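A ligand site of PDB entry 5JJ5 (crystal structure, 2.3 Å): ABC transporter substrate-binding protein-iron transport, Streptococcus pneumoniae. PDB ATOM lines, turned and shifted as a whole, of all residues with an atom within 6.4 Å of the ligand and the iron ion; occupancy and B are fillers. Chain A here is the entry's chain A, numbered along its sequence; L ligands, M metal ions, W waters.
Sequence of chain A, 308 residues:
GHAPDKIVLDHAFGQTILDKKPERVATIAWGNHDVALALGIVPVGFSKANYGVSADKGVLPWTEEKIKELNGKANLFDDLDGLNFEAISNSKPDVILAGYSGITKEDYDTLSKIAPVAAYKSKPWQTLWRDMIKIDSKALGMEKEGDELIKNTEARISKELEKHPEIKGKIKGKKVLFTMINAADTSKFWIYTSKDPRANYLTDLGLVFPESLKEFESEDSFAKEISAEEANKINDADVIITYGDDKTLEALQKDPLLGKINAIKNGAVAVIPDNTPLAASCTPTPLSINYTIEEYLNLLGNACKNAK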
ATOM      1  N   TRP A  30      10.319   0.091  16.536  1.00  0.00           N
ATOM      2  CA  TRP A  30      10.636   1.022  15.464  1.00  0.00           C
ATOM      3  C   TRP A  30       9.809   2.309  15.529  1.00  0.00           C
ATOM      4  O   TRP A  30       8.591   2.280  15.708  1.00  0.00           O
ATOM      5  CB  TRP A  30      10.422   0.347  14.107  1.00  0.00           C
ATOM      6  CG  TRP A  30      10.909   1.148  12.947  1.00  0.00           C
ATOM      7  CD1 TRP A  30      10.216   2.085  12.243  1.00  0.00           C
ATOM      8  CD2 TRP A  30      12.217   1.089  12.359  1.00  0.00           C
ATOM      9  NE1 TRP A  30      10.999   2.617  11.249  1.00  0.00           N
ATOM     10  CE2 TRP A  30      12.237   2.025  11.299  1.00  0.00           C
ATOM     11  CE3 TRP A  30      13.374   0.345  12.616  1.00  0.00           C
ATOM     12  CZ2 TRP A  30      13.363   2.228  10.504  1.00  0.00           C
ATOM     13  CZ3 TRP A  30      14.483   0.549  11.827  1.00  0.00           C
ATOM     14  CH2 TRP A  30      14.478   1.480  10.781  1.00  0.00           C
ATOM     15  N   ASN A  50      17.614  -1.285  13.415  1.00  0.00           N
ATOM     16  CA  ASN A  50      18.140  -2.511  12.822  1.00  0.00           C
ATOM     17  C   ASN A  50      18.085  -2.466  11.305  1.00  0.00           C
ATOM     18  O   ASN A  50      18.254  -3.491  10.645  1.00  0.00           O
ATOM     19  CB  ASN A  50      17.365  -3.720  13.348  1.00  0.00           C
ATOM     20  CG  ASN A  50      15.885  -3.670  12.999  1.00  0.00           C
ATOM     21  OD1 ASN A  50      15.354  -2.626  12.618  1.00  0.00           O
ATOM     22  ND2 ASN A  50      15.212  -4.804  13.138  1.00  0.00           N
ATOM     23  N   TYR A  51      17.866  -1.277  10.759  1.00  0.00           N
ATOM     24  CA  TYR A  51      17.757  -1.101   9.308  1.00  0.00           C
ATOM     25  C   TYR A  51      18.035   0.344   8.915  1.00  0.00           C
ATOM     26  O   TYR A  51      17.562   1.283   9.566  1.00  0.00           O
ATOM     27  CB  TYR A  51      16.354  -1.509   8.829  1.00  0.00           C
ATOM     28  CG  TYR A  51      16.217  -1.557   7.321  1.00  0.00           C
ATOM     29  CD1 TYR A  51      16.699  -2.638   6.601  1.00  0.00           C
ATOM     30  CD2 TYR A  51      15.601  -0.526   6.627  1.00  0.00           C
ATOM     31  CE1 TYR A  51      16.591  -2.697   5.225  1.00  0.00           C
ATOM     32  CE2 TYR A  51      15.480  -0.570   5.248  1.00  0.00           C
ATOM     33  CZ  TYR A  51      15.977  -1.659   4.553  1.00  0.00           C
ATOM     34  OH  TYR A  51      15.859  -1.724   3.185  1.00  0.00           O
ATOM     35  N   TYR A 100       3.990   1.115  17.818  1.00  0.00           N
ATOM     36  CA  TYR A 100       4.385   0.370  16.637  1.00  0.00           C
ATOM     37  C   TYR A 100       5.437  -0.637  17.055  1.00  0.00           C
ATOM     38  O   TYR A 100       6.587  -0.275  17.290  1.00  0.00           O
ATOM     39  CB  TYR A 100       4.919   1.309  15.551  1.00  0.00           C
ATOM     40  CG  TYR A 100       5.215   0.657  14.217  1.00  0.00           C
ATOM     41  CD1 TYR A 100       4.396  -0.341  13.714  1.00  0.00           C
ATOM     42  CD2 TYR A 100       6.302   1.061  13.451  1.00  0.00           C
ATOM     43  CE1 TYR A 100       4.666  -0.936  12.487  1.00  0.00           C
ATOM     44  CE2 TYR A 100       6.571   0.480  12.234  1.00  0.00           C
ATOM     45  CZ  TYR A 100       5.753  -0.511  11.752  1.00  0.00           C
ATOM     46  OH  TYR A 100       6.039  -1.093  10.529  1.00  0.00           O
ATOM     47  N   TRP A 125       3.016  -5.296  14.399  1.00  0.00           N
ATOM     48  CA  TRP A 125       3.469  -4.507  13.251  1.00  0.00           C
ATOM     49  C   TRP A 125       2.333  -4.000  12.369  1.00  0.00           C
ATOM     50  O   TRP A 125       2.552  -3.650  11.213  1.00  0.00           O
ATOM     51  CB  TRP A 125       4.444  -5.321  12.403  1.00  0.00           C
ATOM     52  CG  TRP A 125       5.636  -5.810  13.165  1.00  0.00           C
ATOM     53  CD1 TRP A 125       5.973  -7.117  13.412  1.00  0.00           C
ATOM     54  CD2 TRP A 125       6.643  -5.009  13.793  1.00  0.00           C
ATOM     55  NE1 TRP A 125       7.128  -7.163  14.150  1.00  0.00           N
ATOM     56  CE2 TRP A 125       7.557  -5.889  14.400  1.00  0.00           C
ATOM     57  CE3 TRP A 125       6.847  -3.628  13.898  1.00  0.00           C
ATOM     58  CZ2 TRP A 125       8.675  -5.430  15.103  1.00  0.00           C
ATOM     59  CZ3 TRP A 125       7.964  -3.182  14.601  1.00  0.00           C
ATOM     60  CH2 TRP A 125       8.859  -4.082  15.193  1.00  0.00           C
ATOM     61  N   MET A 180       8.641  -6.765  -1.720  1.00  0.00           N
ATOM     62  CA  MET A 180      10.041  -7.092  -1.524  1.00  0.00           C
ATOM     63  C   MET A 180      10.429  -8.193  -2.498  1.00  0.00           C
ATOM     64  O   MET A 180      10.140  -9.366  -2.265  1.00  0.00           O
ATOM     65  CB  MET A 180      10.343  -7.521  -0.092  1.00  0.00           C
ATOM     66  CG  MET A 180      11.795  -7.958   0.077  1.00  0.00           C
ATOM     67  SD  MET A 180      12.240  -8.434   1.755  1.00  0.00           S
ATOM     68  CE  MET A 180      12.010  -6.882   2.612  1.00  0.00           C
ATOM     69  N   TRP A 190       7.423 -10.952  -1.630  1.00  0.00           N
ATOM     70  CA  TRP A 190       6.486 -10.433  -0.645  1.00  0.00           C
ATOM     71  C   TRP A 190       5.671  -9.269  -1.197  1.00  0.00           C
ATOM     72  O   TRP A 190       6.176  -8.452  -1.958  1.00  0.00           O
ATOM     73  CB  TRP A 190       7.227  -9.961   0.609  1.00  0.00           C
ATOM     74  CG  TRP A 190       7.795 -11.068   1.435  1.00  0.00           C
ATOM     75  CD1 TRP A 190       9.073 -11.555   1.392  1.00  0.00           C
ATOM     76  CD2 TRP A 190       7.100 -11.832   2.424  1.00  0.00           C
ATOM     77  NE1 TRP A 190       9.213 -12.578   2.298  1.00  0.00           N
ATOM     78  CE2 TRP A 190       8.018 -12.768   2.950  1.00  0.00           C
ATOM     79  CE3 TRP A 190       5.799 -11.816   2.921  1.00  0.00           C
ATOM     80  CZ2 TRP A 190       7.673 -13.676   3.942  1.00  0.00           C
ATOM     81  CZ3 TRP A 190       5.454 -12.723   3.913  1.00  0.00           C
ATOM     82  CH2 TRP A 190       6.387 -13.639   4.412  1.00  0.00           C
ATOM     83  N   TYR A 192       3.246  -6.242   0.514  1.00  0.00           N
ATOM     84  CA  TYR A 192       2.766  -5.648   1.757  1.00  0.00           C
ATOM     85  C   TYR A 192       1.317  -5.219   1.599  1.00  0.00           C
ATOM     86  O   TYR A 192       0.954  -4.591   0.604  1.00  0.00           O
ATOM     87  CB  TYR A 192       3.657  -4.477   2.174  1.00  0.00           C
ATOM     88  CG  TYR A 192       5.061  -4.912   2.517  1.00  0.00           C
ATOM     89  CD1 TYR A 192       5.389  -5.341   3.801  1.00  0.00           C
ATOM     90  CD2 TYR A 192       6.071  -4.912   1.557  1.00  0.00           C
ATOM     91  CE1 TYR A 192       6.669  -5.754   4.120  1.00  0.00           C
ATOM     92  CE2 TYR A 192       7.355  -5.310   1.867  1.00  0.00           C
ATOM     93  CZ  TYR A 192       7.655  -5.738   3.143  1.00  0.00           C
ATOM     94  OH  TYR A 192       8.932  -6.143   3.451  1.00  0.00           O
ATOM     95  N   ASP A 196      -0.195  -2.677   6.482  1.00  0.00           N
ATOM     96  CA  ASP A 196       1.180  -2.244   6.716  1.00  0.00           C
ATOM     97  C   ASP A 196       1.343  -0.751   6.488  1.00  0.00           C
ATOM     98  O   ASP A 196       0.886  -0.216   5.490  1.00  0.00           O
ATOM     99  CB  ASP A 196       2.158  -3.016   5.817  1.00  0.00           C
ATOM    100  CG  ASP A 196       3.609  -2.788   6.208  1.00  0.00           C
ATOM    101  OD1 ASP A 196       4.166  -1.737   5.852  1.00  0.00           O
ATOM    102  OD2 ASP A 196       4.180  -3.660   6.888  1.00  0.00           O
ATOM    103  N   ARG A 198       3.796   1.053   5.583  1.00  0.00           N
ATOM    104  CA  ARG A 198       4.595   1.486   4.449  1.00  0.00           C
ATOM    105  C   ARG A 198       3.788   1.402   3.153  1.00  0.00           C
ATOM    106  O   ARG A 198       4.123   2.048   2.161  1.00  0.00           O
ATOM    107  CB  ARG A 198       5.888   0.666   4.350  1.00  0.00           C
ATOM    108  CG  ARG A 198       5.834  -0.534   3.413  1.00  0.00           C
ATOM    109  CD  ARG A 198       6.971  -1.496   3.719  1.00  0.00           C
ATOM    110  NE  ARG A 198       6.743  -2.202   4.979  1.00  0.00           N
ATOM    111  CZ  ARG A 198       7.672  -2.885   5.630  1.00  0.00           C
ATOM    112  NH1 ARG A 198       8.905  -2.953   5.156  1.00  0.00           N
ATOM    113  NH2 ARG A 198       7.367  -3.498   6.765  1.00  0.00           N
ATOM    114  N   PHE A 222       0.797  -8.309   7.753  1.00  0.00           N
ATOM    115  CA  PHE A 222       1.001  -7.048   7.072  1.00  0.00           C
ATOM    116  C   PHE A 222       1.587  -7.293   5.689  1.00  0.00           C
ATOM    117  O   PHE A 222       1.695  -6.372   4.871  1.00  0.00           O
ATOM    118  CB  PHE A 222       1.932  -6.159   7.896  1.00  0.00           C
ATOM    119  CG  PHE A 222       3.189  -6.868   8.336  1.00  0.00           C
ATOM    120  CD1 PHE A 222       4.324  -6.829   7.545  1.00  0.00           C
ATOM    121  CD2 PHE A 222       3.216  -7.575   9.520  1.00  0.00           C
ATOM    122  CE1 PHE A 222       5.477  -7.489   7.946  1.00  0.00           C
ATOM    123  CE2 PHE A 222       4.370  -8.235   9.921  1.00  0.00           C
ATOM    124  CZ  PHE A 222       5.498  -8.188   9.128  1.00  0.00           C
ATOM    125  N   ALA A 223       1.995  -8.536   5.448  1.00  0.00           N
ATOM    126  CA  ALA A 223       2.606  -8.905   4.187  1.00  0.00           C
ATOM    127  C   ALA A 223       2.209 -10.321   3.781  1.00  0.00           C
ATOM    128  O   ALA A 223       1.966 -11.177   4.624  1.00  0.00           O
ATOM    129  CB  ALA A 223       4.123  -8.799   4.275  1.00  0.00           C
ATOM    130  N   LYS A 224       2.152 -10.547   2.472  1.00  0.00           N
ATOM    131  CA  LYS A 224       1.777 -11.842   1.936  1.00  0.00           C
ATOM    132  C   LYS A 224       2.841 -12.321   0.954  1.00  0.00           C
ATOM    133  O   LYS A 224       3.291 -11.556   0.106  1.00  0.00           O
ATOM    134  CB  LYS A 224       0.413 -11.762   1.245  1.00  0.00           C
ATOM    135  CG  LYS A 224      -0.128 -13.089   0.717  1.00  0.00           C
ATOM    136  CD  LYS A 224      -0.714 -13.933   1.829  1.00  0.00           C
ATOM    137  CE  LYS A 224      -1.515 -15.101   1.270  1.00  0.00           C
ATOM    138  NZ  LYS A 224      -0.683 -15.998   0.415  1.00  0.00           N
ATOM    139  N   TYR A 243      12.577  -2.799  -2.440  1.00  0.00           N
ATOM    140  CA  TYR A 243      13.942  -2.530  -2.020  1.00  0.00           C
ATOM    141  C   TYR A 243      14.883  -3.185  -3.024  1.00  0.00           C
ATOM    142  O   TYR A 243      14.540  -4.191  -3.637  1.00  0.00           O
ATOM    143  CB  TYR A 243      14.215  -3.071  -0.616  1.00  0.00           C
ATOM    144  CG  TYR A 243      13.222  -2.633   0.448  1.00  0.00           C
ATOM    145  CD1 TYR A 243      13.317  -1.397   1.054  1.00  0.00           C
ATOM    146  CD2 TYR A 243      12.200  -3.491   0.862  1.00  0.00           C
ATOM    147  CE1 TYR A 243      12.425  -1.001   2.031  1.00  0.00           C
ATOM    148  CE2 TYR A 243      11.307  -3.109   1.840  1.00  0.00           C
ATOM    149  CZ  TYR A 243      11.425  -1.860   2.420  1.00  0.00           C
ATOM    150  OH  TYR A 243      10.528  -1.470   3.387  1.00  0.00           O
ATOM    151  N   ASP A 274      18.328  -0.376  -0.707  1.00  0.00           N
ATOM    152  CA  ASP A 274      18.194  -1.143   0.517  1.00  0.00           C
ATOM    153  C   ASP A 274      19.203  -0.715   1.584  1.00  0.00           C
ATOM    154  O   ASP A 274      20.333  -0.340   1.276  1.00  0.00           O
ATOM    155  CB  ASP A 274      18.349  -2.639   0.220  1.00  0.00           C
ATOM    156  CG  ASP A 274      18.045  -3.516   1.420  1.00  0.00           C
ATOM    157  OD1 ASP A 274      16.858  -3.710   1.742  1.00  0.00           O
ATOM    158  OD2 ASP A 274      19.003  -4.037   2.036  1.00  0.00           O
ATOM    159  N   ALA A 279      15.421   4.071   2.591  1.00  0.00           N
ATOM    160  CA  ALA A 279      14.707   2.813   2.688  1.00  0.00           C
ATOM    161  C   ALA A 279      14.010   2.676   4.034  1.00  0.00           C
ATOM    162  O   ALA A 279      12.883   2.196   4.117  1.00  0.00           O
ATOM    163  CB  ALA A 279      15.660   1.648   2.459  1.00  0.00           C
ATOM    164  N   THR A 283       8.543   3.148   6.145  1.00  0.00           N
ATOM    165  CA  THR A 283       7.585   3.066   7.244  1.00  0.00           C
ATOM    166  C   THR A 283       7.694   4.378   8.008  1.00  0.00           C
ATOM    167  O   THR A 283       8.554   4.526   8.882  1.00  0.00           O
ATOM    168  CB  THR A 283       7.859   1.885   8.188  1.00  0.00           C
ATOM    169  OG1 THR A 283       9.178   2.000   8.741  1.00  0.00           O
ATOM    170  CG2 THR A 283       7.737   0.567   7.441  1.00  0.00           C
HETATM  171  C1  LIG L   1       9.036  -7.634  10.869  1.00  0.00           C
HETATM  172  C2  LIG L   1       9.384  -9.063  11.234  1.00  0.00           C
HETATM  173  C3  LIG L   1       8.518 -10.221  10.782  1.00  0.00           C
HETATM  174  O1  LIG L   1       7.123 -10.329  10.861  1.00  0.00           O
HETATM  175  N1  LIG L   1       8.984 -11.014   9.703  1.00  0.00           N
HETATM  176  C4  LIG L   1       7.888 -11.560   9.007  1.00  0.00           C
HETATM  177  C5  LIG L   1       8.593 -11.679   7.676  1.00  0.00           C
HETATM  178  C6  LIG L   1       8.192 -10.708   6.585  1.00  0.00           C
HETATM  179  C7  LIG L   1       7.771  -9.961   5.345  1.00  0.00           C
HETATM  180  C8  LIG L   1       9.118  -9.604   4.743  1.00  0.00           C
HETATM  181  N2  LIG L   1       9.833  -8.536   5.352  1.00  0.00           N
HETATM  182  O2  LIG L   1       9.214  -7.350   5.600  1.00  0.00           O
HETATM  183  C9  LIG L   1      11.152  -8.775   5.815  1.00  0.00           C
HETATM  184  O3  LIG L   1      11.721  -7.997   6.563  1.00  0.00           O
HETATM  185  C10 LIG L   1      11.693 -10.110   5.331  1.00  0.00           C
HETATM  186  C11 LIG L   1      13.189 -10.018   5.549  1.00  0.00           C
HETATM  187  O4  LIG L   1      14.402  -9.085   4.097  1.00  0.00           O
HETATM  188  C12 LIG L   1      14.408  -9.133   5.498  1.00  0.00           C
HETATM  189  N3  LIG L   1      15.016  -7.855   5.579  1.00  0.00           N
HETATM  190  C13 LIG L   1      15.755  -7.010   4.715  1.00  0.00           C
HETATM  191  C14 LIG L   1      14.951  -5.747   4.880  1.00  0.00           C
HETATM  192  C15 LIG L   1      13.602  -5.166   5.235  1.00  0.00           C
HETATM  193  C16 LIG L   1      13.061  -3.810   4.859  1.00  0.00           C
HETATM  194  C17 LIG L   1      12.536  -3.242   6.152  1.00  0.00           C
HETATM  195  N4  LIG L   1      11.882  -4.261   6.875  1.00  0.00           N
HETATM  196  O5  LIG L   1      10.824  -4.810   6.200  1.00  0.00           O
HETATM  197  C18 LIG L   1      12.298  -4.584   8.182  1.00  0.00           C
HETATM  198  O6  LIG L   1      11.670  -5.580   8.466  1.00  0.00           O
HETATM  199  C19 LIG L   1      13.472  -3.865   8.825  1.00  0.00           C
HETATM  200  C20 LIG L   1      13.453  -4.309  10.274  1.00  0.00           C
HETATM  201  C21 LIG L   1      12.380  -4.284  11.341  1.00  0.00           C
HETATM  202  O7  LIG L   1      12.439  -4.965  12.575  1.00  0.00           O
HETATM  203  N5  LIG L   1      11.653  -3.106  11.662  1.00  0.00           N
HETATM  204  C22 LIG L   1      11.287  -2.293  10.561  1.00  0.00           C
HETATM  205  C23 LIG L   1       9.815  -2.116  10.265  1.00  0.00           C
HETATM  206  C24 LIG L   1       9.189  -2.724  11.499  1.00  0.00           C
HETATM  207  C25 LIG L   1       8.563  -3.709  10.530  1.00  0.00           C
HETATM  208  C26 LIG L   1       7.650  -4.888  10.273  1.00  0.00           C
HETATM  209  N6  LIG L   1       8.048  -6.039   9.386  1.00  0.00           N
HETATM  210  C27 LIG L   1       8.964  -7.127   9.446  1.00  0.00           C
HETATM  211  O8  LIG L   1       9.733  -7.824   8.821  1.00  0.00           O
HETATM  212  O9  LIG L   1       8.523  -5.861   8.114  1.00  0.00           O
HETATM  213 FE    FE M   1      10.246  -6.560   7.219  1.00  0.00          FE
HETATM  214  O   HOH W   1      12.208 -10.738   9.257  1.00  0.00           O
HETATM  215  O   HOH W   2      12.694  -2.655  14.675  1.00  0.00           O
HETATM  216  O   HOH W   3      12.071  -7.361  12.144  1.00  0.00           O
HETATM  217  O   HOH W   4      15.955  -8.888   1.698  1.00  0.00           O
HETATM  218  O   HOH W   5      14.285 -11.397   2.842  1.00  0.00           O
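The iron ion is bound by an oxygen (O9) of the ligand, an oxygen (O2) of the ligand, an oxygen (O8) of the ligand, an oxygen (O5) of the ligand, an oxygen (O6) of the ligand and an oxygen (O3) of the ligand.
The iron ion has six donor atoms within binding distance.
Water W5 lies within hydrogen-bond range of O4 of the ligand and SD of Met 180.
Water W4 bridges an oxygen (O4) of the ligand (2.9 Å) and the side-chain sulfur of Met 180 (3.7 Å).
Water W2 bridges an oxygen (O7) of the ligand and the side-chain amide oxygen (OD1) of Asn 50.
The side-chain sulfur of Met 180 sits close to an oxygen (O4) of the ligand, at 3.3 Å.
CD2 of Trp 30 touches C22 of the ligand, at 3.9 Å.
Tyr 51 touches the ligand (CE1 to C14, 3.5 Å).
Tyr 100 touches the ligand.
CZ3 of Trp 125 touches C24 of the ligand, 3.4 Å away.
Trp 190 touches the ligand (CD2 to C7, 3.5 Å).
Phe 222 touches the ligand.
Ala 223 touches the ligand.
Tyr 243 touches the ligand.
Hydrophobic or aromatic side chains that line the ligand: Trp 30, Tyr 51, Trp 125, Met 180, Trp 190, Tyr 192, Phe 222, Ala 223 and Tyr 243.
The nearest printed residue that does not touch the ligand is Asp 274 (4.2 Å).
No residue comes within 4 Å of the iron ion.
The nearest printed residue that does not touch the iron ion is Tyr 192 (4.01 Å).
The guanidinium group (NH1) of Arg 198 is in hydrogen-bond range of the side-chain hydroxyl (OH) of Tyr 243, at 2.8 Å.
The guanidinium group (NE) of Arg 198 lies within salt-bridge range of the side-chain carboxylate (OD1) of Asp 196, 2.8 Å away.
N of Met 180 is in hydrogen-bond range of O of Trp 190 (3.0 Å).
OD1 of Asp 274 lies within hydrogen-bond range of OH of Tyr 51, 2.7 Å away.
The indole nitrogen (NE1) of Trp 30 lies within hydrogen-bond range of the side-chain hydroxyl (OG1) of Thr 283 (3.2 Å).
O2 of the ligand sits close to OH of Tyr 192 (2.5 Å).
O7 of the ligand lies within hydrogen-bond range of ND2 of Asn 50, 2.8 Å away.
The guanidinium group (NH1) of Arg 198 sits close to an oxygen (O5) of the ligand, at 2.9 Å.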
